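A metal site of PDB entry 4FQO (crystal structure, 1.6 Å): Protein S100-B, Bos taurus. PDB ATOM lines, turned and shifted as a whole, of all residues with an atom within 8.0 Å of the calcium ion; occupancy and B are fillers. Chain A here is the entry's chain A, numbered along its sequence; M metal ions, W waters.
The backbone carbonyl oxygen (O) of Ser 19 binds the calcium ion, 2.3 Å away. The backbone carbonyl oxygen (O) of Asp 24 is bound to the calcium ion, at 2.4 Å. The backbone carbonyl oxygen (O) of Lys 27 is bound to the calcium ion (2.4 Å). Water W1 is bound to the calcium ion, at 2.4 Å. OE1 of Glu 32 binds the calcium ion, at 2.4 Å. O of Glu 22 binds the calcium ion (2.4 Å). The calcium ion is bound by the side-chain carboxylate (OE2) of Glu 32, at 2.4 Å.
O of Phe 15 is in hydrogen-bond range of OG of Ser 19 (3.2 Å). OG of Ser 19 is in hydrogen-bond range of O of Lys 25, at 2.9 Å. OE1 of Glu 32 sits close to N of Lys 29. The side-chain carboxylate (OD2) of Asp 24 lies within salt-bridge range of the side-chain amino group (NZ) of Lys 27 (3.95 Å). OE1 of Glu 22 lies within salt-bridge range of NZ of Lys 29 (3.2 Å). The side-chain carboxylate (OE2) of Glu 22 is in hydrogen-bond range of the side-chain hydroxyl (OG) of Ser 31 (2.6 Å). The backbone NH of Arg 21 sits close to the side-chain carboxylate of Glu 32 (3.5 Å). The backbone NH (N) of His 26 lies within hydrogen-bond range of the side-chain carboxylate (OD1) of Asp 24 (2.8 Å).
Water W1 lies within hydrogen-bond range of OE1 of Glu 68 (2.7 Å) and N of Lys 29 (3.5 Å).
Five residues have an atom within 4 Å of the calcium ion: Ser 19, Glu 22, Asp 24, Lys 27 and Glu 32. Along chain A the residues within 4 Å of the calcium ion span positions 19 to 32. The nearest printed residue that does not touch the calcium ion is Gly 23 (4.3 Å).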
ATOM      1  N   PHE A  15      27.625   7.434 -22.069  1.00  0.00           N
ATOM      2  CA  PHE A  15      27.209   6.226 -21.350  1.00  0.00           C
ATOM      3  C   PHE A  15      27.861   5.017 -21.995  1.00  0.00           C
ATOM      4  O   PHE A  15      28.467   4.205 -21.309  1.00  0.00           O
ATOM      5  CB  PHE A  15      25.706   6.085 -21.344  1.00  0.00           C
ATOM      6  CG  PHE A  15      25.209   4.850 -20.632  1.00  0.00           C
ATOM      7  CD1 PHE A  15      25.140   4.803 -19.241  1.00  0.00           C
ATOM      8  CD2 PHE A  15      24.817   3.742 -21.350  1.00  0.00           C
ATOM      9  CE1 PHE A  15      24.687   3.645 -18.582  1.00  0.00           C
ATOM     10  CE2 PHE A  15      24.373   2.575 -20.696  1.00  0.00           C
ATOM     11  CZ  PHE A  15      24.282   2.547 -19.315  1.00  0.00           C
ATOM     12  N   HIS A  16      27.750   4.928 -23.308  1.00  0.00           N
ATOM     13  CA  HIS A  16      28.304   3.758 -24.012  1.00  0.00           C
ATOM     14  C   HIS A  16      29.810   3.673 -24.051  1.00  0.00           C
ATOM     15  O   HIS A  16      30.383   2.547 -24.118  1.00  0.00           O
ATOM     16  CB  HIS A  16      27.630   3.631 -25.347  1.00  0.00           C
ATOM     17  CG  HIS A  16      26.313   2.948 -25.210  1.00  0.00           C
ATOM     18  ND1 HIS A  16      25.111   3.607 -25.324  1.00  0.00           N
ATOM     19  CD2 HIS A  16      26.026   1.677 -24.837  1.00  0.00           C
ATOM     20  CE1 HIS A  16      24.129   2.754 -25.080  1.00  0.00           C
ATOM     21  NE2 HIS A  16      24.659   1.581 -24.760  1.00  0.00           N
ATOM     22  N   TYR A  18      31.640   4.207 -21.639  1.00  0.00           N
ATOM     23  CA  TYR A  18      32.045   3.608 -20.366  1.00  0.00           C
ATOM     24  C   TYR A  18      31.381   2.271 -20.076  1.00  0.00           C
ATOM     25  O   TYR A  18      32.054   1.363 -19.562  1.00  0.00           O
ATOM     26  CB  TYR A  18      31.897   4.626 -19.222  1.00  0.00           C
ATOM     27  CG  TYR A  18      32.984   5.653 -19.371  1.00  0.00           C
ATOM     28  CD1 TYR A  18      32.782   6.793 -20.159  1.00  0.00           C
ATOM     29  CD2 TYR A  18      34.254   5.422 -18.849  1.00  0.00           C
ATOM     30  CE1 TYR A  18      33.847   7.698 -20.357  1.00  0.00           C
ATOM     31  CE2 TYR A  18      35.281   6.316 -19.026  1.00  0.00           C
ATOM     32  CZ  TYR A  18      35.063   7.457 -19.776  1.00  0.00           C
ATOM     33  OH  TYR A  18      36.110   8.312 -19.968  1.00  0.00           O
ATOM     34  N   SER A  19      30.104   2.138 -20.442  1.00  0.00           N
ATOM     35  CA  SER A  19      29.340   0.914 -20.119  1.00  0.00           C
ATOM     36  C   SER A  19      29.806  -0.340 -20.818  1.00  0.00           C
ATOM     37  O   SER A  19      29.630  -1.454 -20.303  1.00  0.00           O
ATOM     38  CB  SER A  19      27.840   1.139 -20.408  1.00  0.00           C
ATOM     39  OG  SER A  19      27.611   1.122 -21.794  1.00  0.00           O
ATOM     40  N   GLY A  20      30.375  -0.176 -22.004  1.00  0.00           N
ATOM     41  CA  GLY A  20      30.848  -1.303 -22.814  1.00  0.00           C
ATOM     42  C   GLY A  20      32.236  -1.859 -22.515  1.00  0.00           C
ATOM     43  O   GLY A  20      32.681  -2.830 -23.157  1.00  0.00           O
ATOM     44  N   ARG A  21      32.915  -1.257 -21.538  1.00  0.00           N
ATOM     45  CA  ARG A  21      34.291  -1.640 -21.215  1.00  0.00           C
ATOM     46  C   ARG A  21      34.353  -3.021 -20.583  1.00  0.00           C
ATOM     47  O   ARG A  21      35.235  -3.801 -20.908  1.00  0.00           O
ATOM     48  CB  ARG A  21      34.944  -0.575 -20.305  1.00  0.00           C
ATOM     49  CG  ARG A  21      35.132   0.824 -20.942  1.00  0.00           C
ATOM     50  CD  ARG A  21      35.720   1.790 -19.886  1.00  0.00           C
ATOM     51  NE  ARG A  21      36.531   2.975 -20.262  1.00  0.00           N
ATOM     52  CZ  ARG A  21      36.538   3.677 -21.399  1.00  0.00           C
ATOM     53  NH1 ARG A  21      35.784   3.381 -22.451  1.00  0.00           N
ATOM     54  NH2 ARG A  21      37.340   4.737 -21.473  1.00  0.00           N
ATOM     55  N   GLU A  22      33.410  -3.305 -19.678  1.00  0.00           N
ATOM     56  CA  GLU A  22      33.438  -4.495 -18.819  1.00  0.00           C
ATOM     57  C   GLU A  22      32.051  -5.105 -18.665  1.00  0.00           C
ATOM     58  O   GLU A  22      31.055  -4.394 -18.605  1.00  0.00           O
ATOM     59  CB  GLU A  22      33.880  -4.081 -17.425  1.00  0.00           C
ATOM     60  CG  GLU A  22      35.271  -3.478 -17.337  1.00  0.00           C
ATOM     61  CD  GLU A  22      35.577  -3.127 -15.908  1.00  0.00           C
ATOM     62  OE1 GLU A  22      35.844  -4.069 -15.123  1.00  0.00           O
ATOM     63  OE2 GLU A  22      35.470  -1.928 -15.564  1.00  0.00           O
ATOM     64  N   GLY A  23      32.017  -6.429 -18.505  1.00  0.00           N
ATOM     65  CA  GLY A  23      30.796  -7.108 -18.093  1.00  0.00           C
ATOM     66  C   GLY A  23      29.592  -6.780 -18.952  1.00  0.00           C
ATOM     67  O   GLY A  23      29.695  -6.749 -20.203  1.00  0.00           O
ATOM     68  N   ASP A  24      28.462  -6.522 -18.295  1.00  0.00           N
ATOM     69  CA  ASP A  24      27.231  -6.114 -18.995  1.00  0.00           C
ATOM     70  C   ASP A  24      27.516  -4.881 -19.826  1.00  0.00           C
ATOM     71  O   ASP A  24      27.913  -3.838 -19.291  1.00  0.00           O
ATOM     72  CB  ASP A  24      26.116  -5.860 -17.966  1.00  0.00           C
ATOM     73  CG  ASP A  24      24.716  -5.685 -18.602  1.00  0.00           C
ATOM     74  OD1 ASP A  24      24.608  -5.160 -19.729  1.00  0.00           O
ATOM     75  OD2 ASP A  24      23.722  -6.066 -17.939  1.00  0.00           O
ATOM     76  N   LYS A  25      27.375  -4.979 -21.142  1.00  0.00           N
ATOM     77  CA  LYS A  25      27.722  -3.853 -21.974  1.00  0.00           C
ATOM     78  C   LYS A  25      26.686  -2.729 -21.917  1.00  0.00           C
ATOM     79  O   LYS A  25      26.922  -1.630 -22.448  1.00  0.00           O
ATOM     80  CB  LYS A  25      27.940  -4.306 -23.416  1.00  0.00           C
ATOM     81  CG  LYS A  25      29.228  -5.088 -23.586  1.00  0.00           C
ATOM     82  CD  LYS A  25      29.171  -5.917 -24.840  1.00  0.00           C
ATOM     83  CE  LYS A  25      30.412  -6.817 -25.006  1.00  0.00           C
ATOM     84  NZ  LYS A  25      31.654  -6.007 -24.846  1.00  0.00           N
ATOM     85  N   HIS A  26      25.559  -2.987 -21.258  1.00  0.00           N
ATOM     86  CA  HIS A  26      24.470  -2.008 -21.154  1.00  0.00           C
ATOM     87  C   HIS A  26      24.353  -1.359 -19.768  1.00  0.00           C
ATOM     88  O   HIS A  26      23.397  -0.630 -19.490  1.00  0.00           O
ATOM     89  CB  HIS A  26      23.144  -2.670 -21.533  1.00  0.00           C
ATOM     90  CG  HIS A  26      23.175  -3.341 -22.876  1.00  0.00           C
ATOM     91  ND1 HIS A  26      23.422  -2.656 -24.037  1.00  0.00           N
ATOM     92  CD2 HIS A  26      22.973  -4.635 -23.221  1.00  0.00           C
ATOM     93  CE1 HIS A  26      23.387  -3.499 -25.055  1.00  0.00           C
ATOM     94  NE2 HIS A  26      23.107  -4.705 -24.596  1.00  0.00           N
ATOM     95  N   LYS A  27      25.297  -1.648 -18.881  1.00  0.00           N
ATOM     96  CA  LYS A  27      25.277  -1.043 -17.544  1.00  0.00           C
ATOM     97  C   LYS A  27      26.681  -0.619 -17.143  1.00  0.00           C
ATOM     98  O   LYS A  27      27.686  -1.188 -17.611  1.00  0.00           O
ATOM     99  CB  LYS A  27      24.726  -2.025 -16.496  1.00  0.00           C
ATOM    100  CG  LYS A  27      23.305  -2.553 -16.782  1.00  0.00           C
ATOM    101  CD  LYS A  27      22.877  -3.513 -15.699  1.00  0.00           C
ATOM    102  CE  LYS A  27      21.498  -4.064 -15.969  1.00  0.00           C
ATOM    103  NZ  LYS A  27      21.256  -5.184 -14.979  1.00  0.00           N
ATOM    104  N   LEU A  28      26.760   0.376 -16.261  1.00  0.00           N
ATOM    105  CA  LEU A  28      28.020   0.809 -15.674  1.00  0.00           C
ATOM    106  C   LEU A  28      28.192   0.088 -14.344  1.00  0.00           C
ATOM    107  O   LEU A  28      27.430   0.329 -13.408  1.00  0.00           O
ATOM    108  CB  LEU A  28      28.030   2.308 -15.406  1.00  0.00           C
ATOM    109  CG  LEU A  28      27.873   3.221 -16.632  1.00  0.00           C
ATOM    110  CD1 LEU A  28      27.391   4.629 -16.167  1.00  0.00           C
ATOM    111  CD2 LEU A  28      29.154   3.334 -17.408  1.00  0.00           C
ATOM    112  N   LYS A  29      29.187  -0.797 -14.251  1.00  0.00           N
ATOM    113  CA  LYS A  29      29.573  -1.315 -12.938  1.00  0.00           C
ATOM    114  C   LYS A  29      30.408  -0.244 -12.221  1.00  0.00           C
ATOM    115  O   LYS A  29      30.781   0.742 -12.824  1.00  0.00           O
ATOM    116  CB  LYS A  29      30.340  -2.655 -13.028  1.00  0.00           C
ATOM    117  CG  LYS A  29      31.665  -2.606 -13.777  1.00  0.00           C
ATOM    118  CD  LYS A  29      32.156  -4.021 -14.154  1.00  0.00           C
ATOM    119  CE  LYS A  29      32.589  -4.811 -12.953  1.00  0.00           C
ATOM    120  NZ  LYS A  29      34.015  -4.565 -12.569  1.00  0.00           N
ATOM    121  N   LYS A  30      30.704  -0.438 -10.936  1.00  0.00           N
ATOM    122  CA  LYS A  30      31.385   0.611 -10.157  1.00  0.00           C
ATOM    123  C   LYS A  30      32.680   1.085 -10.796  1.00  0.00           C
ATOM    124  O   LYS A  30      32.981   2.273 -10.821  1.00  0.00           O
ATOM    125  CB  LYS A  30      31.612   0.186  -8.699  1.00  0.00           C
ATOM    126  CG  LYS A  30      30.324   0.243  -7.854  1.00  0.00           C
ATOM    127  CD  LYS A  30      30.600  -0.150  -6.394  1.00  0.00           C
ATOM    128  CE  LYS A  30      31.190  -1.545  -6.251  1.00  0.00           C
ATOM    129  NZ  LYS A  30      30.144  -2.567  -6.515  1.00  0.00           N
ATOM    130  N   SER A  31      33.457   0.142 -11.327  1.00  0.00           N
ATOM    131  CA  SER A  31      34.738   0.500 -11.929  1.00  0.00           C
ATOM    132  C   SER A  31      34.523   1.407 -13.140  1.00  0.00           C
ATOM    133  O   SER A  31      35.275   2.378 -13.335  1.00  0.00           O
ATOM    134  CB  SER A  31      35.568  -0.758 -12.293  1.00  0.00           C
ATOM    135  OG  SER A  31      34.791  -1.641 -13.090  1.00  0.00           O
ATOM    136  N   GLU A  32      33.490   1.139 -13.934  1.00  0.00           N
ATOM    137  CA  GLU A  32      33.219   1.962 -15.120  1.00  0.00           C
ATOM    138  C   GLU A  32      32.731   3.353 -14.723  1.00  0.00           C
ATOM    139  O   GLU A  32      33.101   4.366 -15.333  1.00  0.00           O
ATOM    140  CB  GLU A  32      32.196   1.282 -16.025  1.00  0.00           C
ATOM    141  CG  GLU A  32      32.724   0.011 -16.718  1.00  0.00           C
ATOM    142  CD  GLU A  32      31.586  -0.839 -17.279  1.00  0.00           C
ATOM    143  OE1 GLU A  32      30.462  -0.840 -16.734  1.00  0.00           O
ATOM    144  OE2 GLU A  32      31.790  -1.515 -18.279  1.00  0.00           O
ATOM    145  N   LEU A  33      31.871   3.383 -13.706  1.00  0.00           N
ATOM    146  CA  LEU A  33      31.307   4.632 -13.187  1.00  0.00           C
ATOM    147  C   LEU A  33      32.402   5.545 -12.630  1.00  0.00           C
ATOM    148  O   LEU A  33      32.394   6.753 -12.845  1.00  0.00           O
ATOM    149  CB  LEU A  33      30.261   4.313 -12.104  1.00  0.00           C
ATOM    150  CG  LEU A  33      29.608   5.528 -11.467  1.00  0.00           C
ATOM    151  CD1 LEU A  33      28.819   6.374 -12.489  1.00  0.00           C
ATOM    152  CD2 LEU A  33      28.752   5.058 -10.320  1.00  0.00           C
ATOM    153  N   GLU A  68      24.783  -2.052 -10.211  1.00  0.00           N
ATOM    154  CA  GLU A  68      25.237  -1.343 -11.403  1.00  0.00           C
ATOM    155  C   GLU A  68      24.292  -0.223 -11.770  1.00  0.00           C
ATOM    156  O   GLU A  68      23.162  -0.131 -11.262  1.00  0.00           O
ATOM    157  CB  GLU A  68      25.361  -2.310 -12.573  1.00  0.00           C
ATOM    158  CG  GLU A  68      26.261  -3.510 -12.285  1.00  0.00           C
ATOM    159  CD  GLU A  68      26.884  -4.102 -13.503  1.00  0.00           C
ATOM    160  OE1 GLU A  68      27.004  -3.400 -14.511  1.00  0.00           O
ATOM    161  OE2 GLU A  68      27.300  -5.290 -13.438  1.00  0.00           O
ATOM    162  N   CYS A  69      24.761   0.658 -12.648  1.00  0.00           N
ATOM    163  CA  CYS A  69      23.952   1.802 -13.061  1.00  0.00           C
ATOM    164  C   CYS A  69      23.539   1.609 -14.512  1.00  0.00           C
ATOM    165  O   CYS A  69      24.388   1.635 -15.411  1.00  0.00           O
ATOM    166  CB  CYS A  69      24.755   3.077 -12.852  1.00  0.00           C
ATOM    167  SG  CYS A  69      23.947   4.593 -13.474  1.00  0.00           S
HETATM  168 CA    CA M   1      29.557  -2.513 -18.247  1.00  0.00          CA
HETATM  169  O   HOH W   1      29.133  -3.663 -16.197  1.00  0.00           O
